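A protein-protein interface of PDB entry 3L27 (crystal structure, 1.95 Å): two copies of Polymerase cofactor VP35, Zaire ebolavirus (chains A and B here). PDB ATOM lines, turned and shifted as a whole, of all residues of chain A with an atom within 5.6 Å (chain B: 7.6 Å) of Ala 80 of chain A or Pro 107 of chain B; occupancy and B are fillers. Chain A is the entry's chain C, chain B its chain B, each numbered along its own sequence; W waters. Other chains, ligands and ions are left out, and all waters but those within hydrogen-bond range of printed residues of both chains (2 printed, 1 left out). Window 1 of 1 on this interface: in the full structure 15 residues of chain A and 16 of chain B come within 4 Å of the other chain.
The side-chain hydroxyl of Ser 106 of chain B sits at hydrogen-bond distance from the backbone carbonyl oxygen of Pro 81 of chain A (2.6 Å). O of Asp 78 of chain A is in hydrogen-bond range of N of Ala 80 of chain B (2.9 Å). N of Ala 80 of chain A sits at hydrogen-bond distance from O of Asp 78 of chain B. The backbone carbonyl oxygen of Pro 81 of chain B is in hydrogen-bond range of the side-chain hydroxyl of Ser 106 of chain A. The backbone carbonyl oxygen (O) of Pro 81 of chain A sits at hydrogen-bond distance from the side-chain amino group (NZ) of Lys 108 of chain B (2.9 Å).
NZ of Lys 108 of chain B lies within hydrogen-bond range of O of Ser 106 of chain B (3.0 Å). The backbone carbonyl oxygen (O) of Ala 79 of chain B sits at hydrogen-bond distance from the backbone NH (N) of Ile 109 of chain B (2.7 Å). The side-chain carboxylate (OD2) of Asp 110 of chain B lies within hydrogen-bond range of the backbone NH (N) of Asp 78 of chain B, at 3.1 Å. N of Trp 113 of chain B is in hydrogen-bond range of O of Lys 108 of chain B (3.3 Å). The backbone NH of Trp 113 of chain A is in hydrogen-bond range of the backbone carbonyl oxygen of Lys 108 of chain A (3.2 Å). The backbone NH (N) of Ile 109 of chain A lies within hydrogen-bond range of the backbone carbonyl oxygen (O) of Ala 79 of chain A.
Asp 78 of chain B touches Leu 38 of chain A. Asp 78 of chain B touches Ala 79 of chain A (O to CA, 3.6 Å). Ala 80 of chain A touches Pro 107 of chain B (CB to O, 3.9 Å). Ala 80 of chain A touches Lys 108 of chain B. CG1 of Val 103 of chain B touches O of Pro 105 of chain A, at 3.7 Å. CD of Pro 107 of chain B touches O of Pro 105 of chain A, at 3.2 Å. OG of Ser 106 of chain A touches CB of Ala 80 of chain B (3.3 Å). Ser 106 of chain A touches Val 83 of chain B. Pro 107 of chain A touches Ala 80 of chain B. CG of Lys 108 of chain A touches CB of Ala 80 of chain B, at 3.8 Å.
Printed residues of chain B within 4 Å of Ala 79 of chain A: Asp 78 (3.6 Å). Ala 80 of chain A touches just these residues of chain B: Asp 78 (2.7 Å), Ser 106 (3.4 Å), Pro 107 (3.9 Å) and Lys 108 (3.9 Å). Printed residues of chain B within 4 Å of Ser 106 of chain A: Ala 80, Pro 81 and Val 83. Printed residues of chain A within 4 Å of Asp 78 of chain B: Leu 38 (3.4 Å), Ala 79 (3.6 Å) and Ala 80 (2.7 Å). Printed residues of chain A within 4 Å of Ala 79 of chain B: Asp 78 (3.3 Å). Of the printed residues of chain A, Pro 107 of chain B touches Ala 80 and Pro 105. The nearest residue of chain A that does not touch Pro 107 of chain B is Pro 107 of chain A (4.4 Å). The nearest printed residue of chain A that does not touch Ala 79 of chain B is Ala 80 of chain A (4.5 Å).
Of the 12 printed residues of chain A, 9 touch a printed residue of chain B. Printed residues of chain A that touch a printed residue of chain B: Leu 38, Asp 78, Ala 79, Ala 80, Pro 81, Pro 105, Ser 106, Pro 107 and Lys 108. Hydrophobic or aromatic side chains of chain B within 4 Å of the printed part of chain A: Ala 79, Ala 80, Pro 81, Val 83, Val 103 and Pro 107.
Ala 80 of chain A touches Pro 107 of chain B, and with the chains exchanged Pro 107 of chain A touches Ala 80 of chain B. Ala 80 of chain A touches Lys 108 of chain B, and with the chains exchanged Lys 108 of chain A touches Ala 80 of chain B. Pro 105 of chain A touches Pro 107 of chain B, but with the chains exchanged Pro 107 of chain A does not touch Pro 105 of chain B (5.2 Å). Pro 107 of chain A touches Ser 106 of chain B, but with the chains exchanged Ser 106 of chain A does not touch Pro 107 of chain B (4.6 Å). 10 positions are printed for both chains. Of the 18 pairs that touch across the chains among the printed residues, 12 have their exchanged pair printed and touching as well.
Water W1 lies within hydrogen-bond range of O of Pro 105 of chain A (2.8 Å), O of Pro 104 of chain B (3.0 Å) and N of Ser 106 of chain B (3.2 Å). Water W2 lies within hydrogen-bond range of O of Pro 107 of chain B (2.8 Å) and O of Pro 107 of chain A (3.2 Å).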
ATOM      1  N   LEU A  38      10.576   6.046  19.704  1.00  0.00           N
ATOM      2  CA  LEU A  38      11.205   5.168  20.701  1.00  0.00           C
ATOM      3  C   LEU A  38      10.801   5.551  22.135  1.00  0.00           C
ATOM      4  O   LEU A  38      10.611   4.663  22.972  1.00  0.00           O
ATOM      5  CB  LEU A  38      12.731   5.207  20.580  1.00  0.00           C
ATOM      6  CG  LEU A  38      13.311   4.229  19.577  1.00  0.00           C
ATOM      7  CD1 LEU A  38      14.741   4.594  19.250  1.00  0.00           C
ATOM      8  CD2 LEU A  38      13.214   2.788  20.130  1.00  0.00           C
ATOM      9  N   ASP A  78      22.350   1.372  22.990  1.00  0.00           N
ATOM     10  CA  ASP A  78      22.449   0.387  21.907  1.00  0.00           C
ATOM     11  C   ASP A  78      21.389   0.420  20.800  1.00  0.00           C
ATOM     12  O   ASP A  78      21.396  -0.447  19.947  1.00  0.00           O
ATOM     13  CB  ASP A  78      22.625  -1.049  22.452  1.00  0.00           C
ATOM     14  CG  ASP A  78      23.238  -1.957  21.420  1.00  0.00           C
ATOM     15  OD1 ASP A  78      22.742  -3.090  21.171  1.00  0.00           O
ATOM     16  OD2 ASP A  78      24.223  -1.479  20.806  1.00  0.00           O
ATOM     17  N   ALA A  79      20.507   1.409  20.762  1.00  0.00           N
ATOM     18  CA  ALA A  79      19.388   1.363  19.796  1.00  0.00           C
ATOM     19  C   ALA A  79      19.843   1.612  18.367  1.00  0.00           C
ATOM     20  O   ALA A  79      20.628   2.519  18.096  1.00  0.00           O
ATOM     21  CB  ALA A  79      18.255   2.339  20.201  1.00  0.00           C
ATOM     22  N   ALA A  80      19.354   0.804  17.441  1.00  0.00           N
ATOM     23  CA  ALA A  80      19.731   0.961  16.024  1.00  0.00           C
ATOM     24  C   ALA A  80      18.682   1.801  15.313  1.00  0.00           C
ATOM     25  O   ALA A  80      17.495   1.705  15.661  1.00  0.00           O
ATOM     26  CB  ALA A  80      19.823  -0.426  15.367  1.00  0.00           C
ATOM     27  N   PRO A  81      19.084   2.561  14.271  1.00  0.00           N
ATOM     28  CA  PRO A  81      18.127   3.440  13.598  1.00  0.00           C
ATOM     29  C   PRO A  81      17.032   2.660  12.850  1.00  0.00           C
ATOM     30  O   PRO A  81      17.267   1.500  12.442  1.00  0.00           O
ATOM     31  CB  PRO A  81      19.007   4.221  12.600  1.00  0.00           C
ATOM     32  CG  PRO A  81      20.227   3.352  12.363  1.00  0.00           C
ATOM     33  CD  PRO A  81      20.445   2.677  13.703  1.00  0.00           C
ATOM     34  N   PRO A  82      15.860   3.291  12.638  1.00  0.00           N
ATOM     35  CA  PRO A  82      14.868   2.642  11.783  1.00  0.00           C
ATOM     36  C   PRO A  82      15.282   2.687  10.318  1.00  0.00           C
ATOM     37  O   PRO A  82      16.034   3.569   9.920  1.00  0.00           O
ATOM     38  CB  PRO A  82      13.624   3.523  11.962  1.00  0.00           C
ATOM     39  CG  PRO A  82      14.150   4.851  12.392  1.00  0.00           C
ATOM     40  CD  PRO A  82      15.396   4.607  13.151  1.00  0.00           C
ATOM     41  N   PRO A 105      28.105  -1.661   9.337  1.00  0.00           N
ATOM     42  CA  PRO A 105      27.484  -2.952   9.702  1.00  0.00           C
ATOM     43  C   PRO A 105      26.393  -2.852  10.771  1.00  0.00           C
ATOM     44  O   PRO A 105      25.271  -3.413  10.616  1.00  0.00           O
ATOM     45  CB  PRO A 105      28.677  -3.760  10.245  1.00  0.00           C
ATOM     46  CG  PRO A 105      29.857  -3.246   9.428  1.00  0.00           C
ATOM     47  CD  PRO A 105      29.586  -1.752   9.333  1.00  0.00           C
ATOM     48  N   SER A 106      26.709  -2.152  11.847  1.00  0.00           N
ATOM     49  CA  SER A 106      25.801  -2.134  13.004  1.00  0.00           C
ATOM     50  C   SER A 106      25.556  -0.680  13.478  1.00  0.00           C
ATOM     51  O   SER A 106      26.057  -0.290  14.526  1.00  0.00           O
ATOM     52  CB  SER A 106      26.383  -3.047  14.095  1.00  0.00           C
ATOM     53  OG  SER A 106      25.531  -3.191  15.220  1.00  0.00           O
ATOM     54  N   PRO A 107      24.796   0.127  12.687  1.00  0.00           N
ATOM     55  CA  PRO A 107      24.612   1.512  13.065  1.00  0.00           C
ATOM     56  C   PRO A 107      23.834   1.678  14.386  1.00  0.00           C
ATOM     57  O   PRO A 107      22.926   0.867  14.684  1.00  0.00           O
ATOM     58  CB  PRO A 107      23.790   2.089  11.926  1.00  0.00           C
ATOM     59  CG  PRO A 107      23.081   0.849  11.318  1.00  0.00           C
ATOM     60  CD  PRO A 107      24.099  -0.197  11.430  1.00  0.00           C
ATOM     61  N   LYS A 108      24.208   2.708  15.152  1.00  0.00           N
ATOM     62  CA  LYS A 108      23.522   3.064  16.420  1.00  0.00           C
ATOM     63  C   LYS A 108      23.063   4.508  16.349  1.00  0.00           C
ATOM     64  O   LYS A 108      23.788   5.370  15.851  1.00  0.00           O
ATOM     65  CB  LYS A 108      24.475   2.911  17.599  1.00  0.00           C
ATOM     66  CG  LYS A 108      24.778   1.438  18.015  1.00  0.00           C
ATOM     67  CD  LYS A 108      25.694   1.419  19.235  1.00  0.00           C
ATOM     68  CE  LYS A 108      27.124   1.808  18.830  1.00  0.00           C
ATOM     69  NZ  LYS A 108      28.128   2.004  19.958  1.00  0.00           N
ATOM     70  N   ILE A 109      21.874   4.794  16.875  1.00  0.00           N
ATOM     71  CA  ILE A 109      21.350   6.182  16.921  1.00  0.00           C
ATOM     72  C   ILE A 109      22.273   7.088  17.758  1.00  0.00           C
ATOM     73  O   ILE A 109      22.518   8.224  17.378  1.00  0.00           O
ATOM     74  CB  ILE A 109      19.901   6.176  17.507  1.00  0.00           C
ATOM     75  CG1 ILE A 109      18.967   5.335  16.593  1.00  0.00           C
ATOM     76  CG2 ILE A 109      19.377   7.637  17.824  1.00  0.00           C
ATOM     77  CD1 ILE A 109      17.627   5.021  17.291  1.00  0.00           C
ATOM     78  N   TRP A 113      23.693   7.878  13.826  1.00  0.00           N
ATOM     79  CA  TRP A 113      22.948   7.284  12.676  1.00  0.00           C
ATOM     80  C   TRP A 113      21.458   7.417  12.974  1.00  0.00           C
ATOM     81  O   TRP A 113      20.870   6.654  13.763  1.00  0.00           O
ATOM     82  CB  TRP A 113      23.361   5.814  12.439  1.00  0.00           C
ATOM     83  CG  TRP A 113      24.813   5.688  12.046  1.00  0.00           C
ATOM     84  CD1 TRP A 113      25.846   5.330  12.843  1.00  0.00           C
ATOM     85  CD2 TRP A 113      25.385   5.990  10.745  1.00  0.00           C
ATOM     86  NE1 TRP A 113      27.024   5.370  12.129  1.00  0.00           N
ATOM     87  CE2 TRP A 113      26.768   5.775  10.844  1.00  0.00           C
ATOM     88  CE3 TRP A 113      24.847   6.435   9.519  1.00  0.00           C
ATOM     89  CZ2 TRP A 113      27.646   5.968   9.758  1.00  0.00           C
ATOM     90  CZ3 TRP A 113      25.719   6.608   8.426  1.00  0.00           C
ATOM     91  CH2 TRP A 113      27.107   6.372   8.560  1.00  0.00           C
ATOM     92  N   GLN B  77      15.547  -4.325  22.652  1.00  0.00           N
ATOM     93  CA  GLN B  77      14.539  -3.762  21.780  1.00  0.00           C
ATOM     94  C   GLN B  77      15.234  -2.833  20.787  1.00  0.00           C
ATOM     95  O   GLN B  77      15.935  -1.909  21.194  1.00  0.00           O
ATOM     96  CB  GLN B  77      13.500  -3.026  22.642  1.00  0.00           C
ATOM     97  CG  GLN B  77      12.635  -1.951  21.979  1.00  0.00           C
ATOM     98  CD  GLN B  77      11.587  -1.400  22.945  1.00  0.00           C
ATOM     99  OE1 GLN B  77      11.642  -1.661  24.152  1.00  0.00           O
ATOM    100  NE2 GLN B  77      10.626  -0.642  22.422  1.00  0.00           N
ATOM    101  N   ASP B  78      15.097  -3.133  19.496  1.00  0.00           N
ATOM    102  CA  ASP B  78      15.825  -2.449  18.409  1.00  0.00           C
ATOM    103  C   ASP B  78      17.345  -2.406  18.577  1.00  0.00           C
ATOM    104  O   ASP B  78      17.995  -1.485  18.065  1.00  0.00           O
ATOM    105  CB  ASP B  78      15.318  -0.994  18.226  1.00  0.00           C
ATOM    106  CG  ASP B  78      13.875  -0.928  17.776  1.00  0.00           C
ATOM    107  OD1 ASP B  78      13.331  -1.940  17.277  1.00  0.00           O
ATOM    108  OD2 ASP B  78      13.277   0.172  17.899  1.00  0.00           O
ATOM    109  N   ALA B  79      17.913  -3.373  19.286  1.00  0.00           N
ATOM    110  CA  ALA B  79      19.330  -3.305  19.647  1.00  0.00           C
ATOM    111  C   ALA B  79      20.262  -3.661  18.485  1.00  0.00           C
ATOM    112  O   ALA B  79      20.078  -4.671  17.809  1.00  0.00           O
ATOM    113  CB  ALA B  79      19.614  -4.211  20.828  1.00  0.00           C
ATOM    114  N   ALA B  80      21.265  -2.827  18.273  1.00  0.00           N
ATOM    115  CA  ALA B  80      22.312  -3.079  17.296  1.00  0.00           C
ATOM    116  C   ALA B  80      23.074  -4.253  17.862  1.00  0.00           C
ATOM    117  O   ALA B  80      23.397  -4.275  19.067  1.00  0.00           O
ATOM    118  CB  ALA B  80      23.216  -1.863  17.145  1.00  0.00           C
ATOM    119  N   PRO B  81      23.305  -5.281  17.028  1.00  0.00           N
ATOM    120  CA  PRO B  81      24.124  -6.432  17.430  1.00  0.00           C
ATOM    121  C   PRO B  81      25.605  -6.046  17.479  1.00  0.00           C
ATOM    122  O   PRO B  81      26.019  -5.122  16.766  1.00  0.00           O
ATOM    123  CB  PRO B  81      23.886  -7.469  16.312  1.00  0.00           C
ATOM    124  CG  PRO B  81      23.187  -6.786  15.214  1.00  0.00           C
ATOM    125  CD  PRO B  81      22.774  -5.397  15.659  1.00  0.00           C
ATOM    126  N   VAL B  83      29.613  -6.132  16.783  1.00  0.00           N
ATOM    127  CA  VAL B  83      30.442  -6.534  15.650  1.00  0.00           C
ATOM    128  C   VAL B  83      31.658  -7.251  16.198  1.00  0.00           C
ATOM    129  O   VAL B  83      32.358  -6.730  17.050  1.00  0.00           O
ATOM    130  CB  VAL B  83      30.889  -5.342  14.796  1.00  0.00           C
ATOM    131  CG1 VAL B  83      31.745  -5.828  13.614  1.00  0.00           C
ATOM    132  CG2 VAL B  83      29.669  -4.595  14.269  1.00  0.00           C
ATOM    133  N   PRO B 102      23.713 -12.369   4.643  1.00  0.00           N
ATOM    134  CA  PRO B 102      24.066 -10.987   4.357  1.00  0.00           C
ATOM    135  C   PRO B 102      23.450 -10.059   5.406  1.00  0.00           C
ATOM    136  O   PRO B 102      22.307 -10.280   5.820  1.00  0.00           O
ATOM    137  CB  PRO B 102      23.444 -10.758   2.974  1.00  0.00           C
ATOM    138  CG  PRO B 102      23.431 -12.088   2.371  1.00  0.00           C
ATOM    139  CD  PRO B 102      23.026 -12.983   3.489  1.00  0.00           C
ATOM    140  N   VAL B 103      24.215  -9.063   5.857  1.00  0.00           N
ATOM    141  CA  VAL B 103      23.752  -8.144   6.897  1.00  0.00           C
ATOM    142  C   VAL B 103      22.812  -7.137   6.260  1.00  0.00           C
ATOM    143  O   VAL B 103      23.172  -6.527   5.268  1.00  0.00           O
ATOM    144  CB  VAL B 103      24.936  -7.401   7.561  1.00  0.00           C
ATOM    145  CG1 VAL B 103      24.440  -6.403   8.634  1.00  0.00           C
ATOM    146  CG2 VAL B 103      25.877  -8.420   8.209  1.00  0.00           C
ATOM    147  N   PRO B 104      21.600  -6.956   6.823  1.00  0.00           N
ATOM    148  CA  PRO B 104      20.657  -5.986   6.278  1.00  0.00           C
ATOM    149  C   PRO B 104      21.077  -4.606   6.763  1.00  0.00           C
ATOM    150  O   PRO B 104      22.011  -4.511   7.551  1.00  0.00           O
ATOM    151  CB  PRO B 104      19.350  -6.370   6.988  1.00  0.00           C
ATOM    152  CG  PRO B 104      19.774  -6.843   8.283  1.00  0.00           C
ATOM    153  CD  PRO B 104      21.049  -7.612   8.025  1.00  0.00           C
ATOM    154  N   PRO B 105      20.405  -3.540   6.292  1.00  0.00           N
ATOM    155  CA  PRO B 105      20.686  -2.232   6.828  1.00  0.00           C
ATOM    156  C   PRO B 105      20.181  -2.151   8.276  1.00  0.00           C
ATOM    157  O   PRO B 105      19.043  -2.534   8.577  1.00  0.00           O
ATOM    158  CB  PRO B 105      19.909  -1.295   5.890  1.00  0.00           C
ATOM    159  CG  PRO B 105      18.860  -2.107   5.237  1.00  0.00           C
ATOM    160  CD  PRO B 105      19.425  -3.512   5.185  1.00  0.00           C
ATOM    161  N   SER B 106      21.010  -1.723   9.206  1.00  0.00           N
ATOM    162  CA  SER B 106      20.509  -1.609  10.585  1.00  0.00           C
ATOM    163  C   SER B 106      19.897  -2.921  11.176  1.00  0.00           C
ATOM    164  O   SER B 106      18.703  -2.991  11.505  1.00  0.00           O
ATOM    165  CB  SER B 106      19.518  -0.446  10.687  1.00  0.00           C
ATOM    166  OG  SER B 106      19.357  -0.065  12.036  1.00  0.00           O
ATOM    167  N   PRO B 107      20.718  -3.969  11.317  1.00  0.00           N
ATOM    168  CA  PRO B 107      20.243  -5.200  11.990  1.00  0.00           C
ATOM    169  C   PRO B 107      19.844  -4.940  13.469  1.00  0.00           C
ATOM    170  O   PRO B 107      20.423  -4.033  14.106  1.00  0.00           O
ATOM    171  CB  PRO B 107      21.442  -6.124  11.894  1.00  0.00           C
ATOM    172  CG  PRO B 107      22.627  -5.204  11.691  1.00  0.00           C
ATOM    173  CD  PRO B 107      22.121  -4.073  10.882  1.00  0.00           C
ATOM    174  N   LYS B 108      18.845  -5.698  13.963  1.00  0.00           N
ATOM    175  CA  LYS B 108      18.311  -5.588  15.323  1.00  0.00           C
ATOM    176  C   LYS B 108      18.353  -6.935  15.971  1.00  0.00           C
ATOM    177  O   LYS B 108      17.929  -7.941  15.368  1.00  0.00           O
ATOM    178  CB  LYS B 108      16.831  -5.188  15.313  1.00  0.00           C
ATOM    179  CG  LYS B 108      16.425  -4.029  14.368  1.00  0.00           C
ATOM    180  CD  LYS B 108      16.671  -2.719  14.893  1.00  0.00           C
ATOM    181  CE  LYS B 108      15.961  -1.586  14.068  1.00  0.00           C
ATOM    182  NZ  LYS B 108      16.588  -1.269  12.724  1.00  0.00           N
ATOM    183  N   ILE B 109      18.788  -6.972  17.221  1.00  0.00           N
ATOM    184  CA  ILE B 109      18.893  -8.274  17.918  1.00  0.00           C
ATOM    185  C   ILE B 109      17.528  -8.923  18.106  1.00  0.00           C
ATOM    186  O   ILE B 109      17.407 -10.165  17.954  1.00  0.00           O
ATOM    187  CB  ILE B 109      19.605  -8.163  19.278  1.00  0.00           C
ATOM    188  CG1 ILE B 109      21.061  -7.720  19.059  1.00  0.00           C
ATOM    189  CG2 ILE B 109      19.512  -9.534  20.112  1.00  0.00           C
ATOM    190  CD1 ILE B 109      21.725  -7.196  20.326  1.00  0.00           C
ATOM    191  N   ASP B 110      16.513  -8.122  18.429  1.00  0.00           N
ATOM    192  CA  ASP B 110      15.152  -8.665  18.609  1.00  0.00           C
ATOM    193  C   ASP B 110      14.490  -9.104  17.297  1.00  0.00           C
ATOM    194  O   ASP B 110      13.377  -9.628  17.324  1.00  0.00           O
ATOM    195  CB  ASP B 110      14.233  -7.695  19.420  1.00  0.00           C
ATOM    196  CG  ASP B 110      14.092  -6.328  18.779  1.00  0.00           C
ATOM    197  OD1 ASP B 110      14.901  -5.941  17.918  1.00  0.00           O
ATOM    198  OD2 ASP B 110      13.187  -5.603  19.199  1.00  0.00           O
ATOM    199  N   ARG B 111      15.178  -8.916  16.166  1.00  0.00           N
ATOM    200  CA  ARG B 111      14.766  -9.499  14.897  1.00  0.00           C
ATOM    201  C   ARG B 111      15.619 -10.731  14.503  1.00  0.00           C
ATOM    202  O   ARG B 111      15.512 -11.224  13.378  1.00  0.00           O
ATOM    203  CB  ARG B 111      14.721  -8.442  13.780  1.00  0.00           C
ATOM    204  CG  ARG B 111      13.698  -7.306  14.073  1.00  0.00           C
ATOM    205  CD  ARG B 111      13.491  -6.386  12.881  1.00  0.00           C
ATOM    206  NE  ARG B 111      12.804  -5.166  13.281  1.00  0.00           N
ATOM    207  CZ  ARG B 111      12.358  -4.249  12.428  1.00  0.00           C
ATOM    208  NH1 ARG B 111      12.550  -4.427  11.120  1.00  0.00           N
ATOM    209  NH2 ARG B 111      11.721  -3.165  12.876  1.00  0.00           N
ATOM    210  N   GLY B 112      16.410 -11.250  15.446  1.00  0.00           N
ATOM    211  CA  GLY B 112      17.193 -12.480  15.210  1.00  0.00           C
ATOM    212  C   GLY B 112      18.612 -12.246  14.710  1.00  0.00           C
ATOM    213  O   GLY B 112      19.283 -13.192  14.377  1.00  0.00           O
ATOM    214  N   TRP B 113      19.055 -10.986  14.637  1.00  0.00           N
ATOM    215  CA  TRP B 113      20.454 -10.704  14.258  1.00  0.00           C
ATOM    216  C   TRP B 113      21.304 -10.705  15.518  1.00  0.00           C
ATOM    217  O   TRP B 113      21.353  -9.718  16.247  1.00  0.00           O
ATOM    218  CB  TRP B 113      20.580  -9.403  13.475  1.00  0.00           C
ATOM    219  CG  TRP B 113      19.830  -9.473  12.151  1.00  0.00           C
ATOM    220  CD1 TRP B 113      18.580  -8.940  11.867  1.00  0.00           C
ATOM    221  CD2 TRP B 113      20.260 -10.152  10.970  1.00  0.00           C
ATOM    222  NE1 TRP B 113      18.227  -9.248  10.559  1.00  0.00           N
ATOM    223  CE2 TRP B 113      19.235 -10.010  10.001  1.00  0.00           C
ATOM    224  CE3 TRP B 113      21.421 -10.902  10.639  1.00  0.00           C
ATOM    225  CZ2 TRP B 113      19.345 -10.561   8.710  1.00  0.00           C
ATOM    226  CZ3 TRP B 113      21.535 -11.435   9.359  1.00  0.00           C
ATOM    227  CH2 TRP B 113      20.504 -11.270   8.413  1.00  0.00           C
ATOM    228  N   VAL B 114      21.946 -11.844  15.766  1.00  0.00           N
ATOM    229  CA  VAL B 114      22.683 -12.104  16.999  1.00  0.00           C
ATOM    230  C   VAL B 114      23.969 -11.253  17.080  1.00  0.00           C
ATOM    231  O   VAL B 114      24.313 -10.654  18.138  1.00  0.00           O
ATOM    232  CB  VAL B 114      23.038 -13.617  17.097  1.00  0.00           C
ATOM    233  CG1 VAL B 114      23.770 -13.901  18.415  1.00  0.00           C
ATOM    234  CG2 VAL B 114      21.758 -14.475  17.073  1.00  0.00           C
ATOM    235  N   CYS B 115      24.727 -11.261  15.987  1.00  0.00           N
ATOM    236  CA  CYS B 115      25.967 -10.497  15.915  1.00  0.00           C
ATOM    237  C   CYS B 115      26.311 -10.333  14.438  1.00  0.00           C
ATOM    238  O   CYS B 115      25.662 -10.942  13.561  1.00  0.00           O
ATOM    239  CB  CYS B 115      27.111 -11.188  16.693  1.00  0.00           C
ATOM    240  SG  CYS B 115      27.641 -12.783  15.979  1.00  0.00           S
ATOM    241  N   VAL B 116      27.312  -9.510  14.166  1.00  0.00           N
ATOM    242  CA  VAL B 116      27.840  -9.366  12.853  1.00  0.00           C
ATOM    243  C   VAL B 116      29.318  -9.712  12.926  1.00  0.00           C
ATOM    244  O   VAL B 116      30.050  -9.153  13.735  1.00  0.00           O
ATOM    245  CB  VAL B 116      27.702  -7.890  12.337  1.00  0.00           C
ATOM    246  CG1 VAL B 116      28.501  -7.694  11.022  1.00  0.00           C
ATOM    247  CG2 VAL B 116      26.247  -7.509  12.183  1.00  0.00           C
ATOM    248  N   GLY B 126      26.173 -11.814   8.890  1.00  0.00           N
ATOM    249  CA  GLY B 126      25.246 -11.684  10.019  1.00  0.00           C
ATOM    250  C   GLY B 126      24.994 -13.076  10.596  1.00  0.00           C
ATOM    251  O   GLY B 126      24.855 -14.028   9.830  1.00  0.00           O
ATOM    252  N   LEU B 127      24.993 -13.220  11.917  1.00  0.00           N
ATOM    253  CA  LEU B 127      24.551 -14.467  12.522  1.00  0.00           C
ATOM    254  C   LEU B 127      23.038 -14.324  12.754  1.00  0.00           C
ATOM    255  O   LEU B 127      22.612 -13.415  13.488  1.00  0.00           O
ATOM    256  CB  LEU B 127      25.280 -14.711  13.865  1.00  0.00           C
ATOM    257  CG  LEU B 127      25.048 -16.081  14.513  1.00  0.00           C
ATOM    258  CD1 LEU B 127      25.447 -17.202  13.561  1.00  0.00           C
ATOM    259  CD2 LEU B 127      25.811 -16.211  15.813  1.00  0.00           C
HETATM  260  O   HOH W   1      24.018  -2.428   8.335  1.00  0.00           O
HETATM  261  O   HOH W   2      22.345  -2.034  13.458  1.00  0.00           O
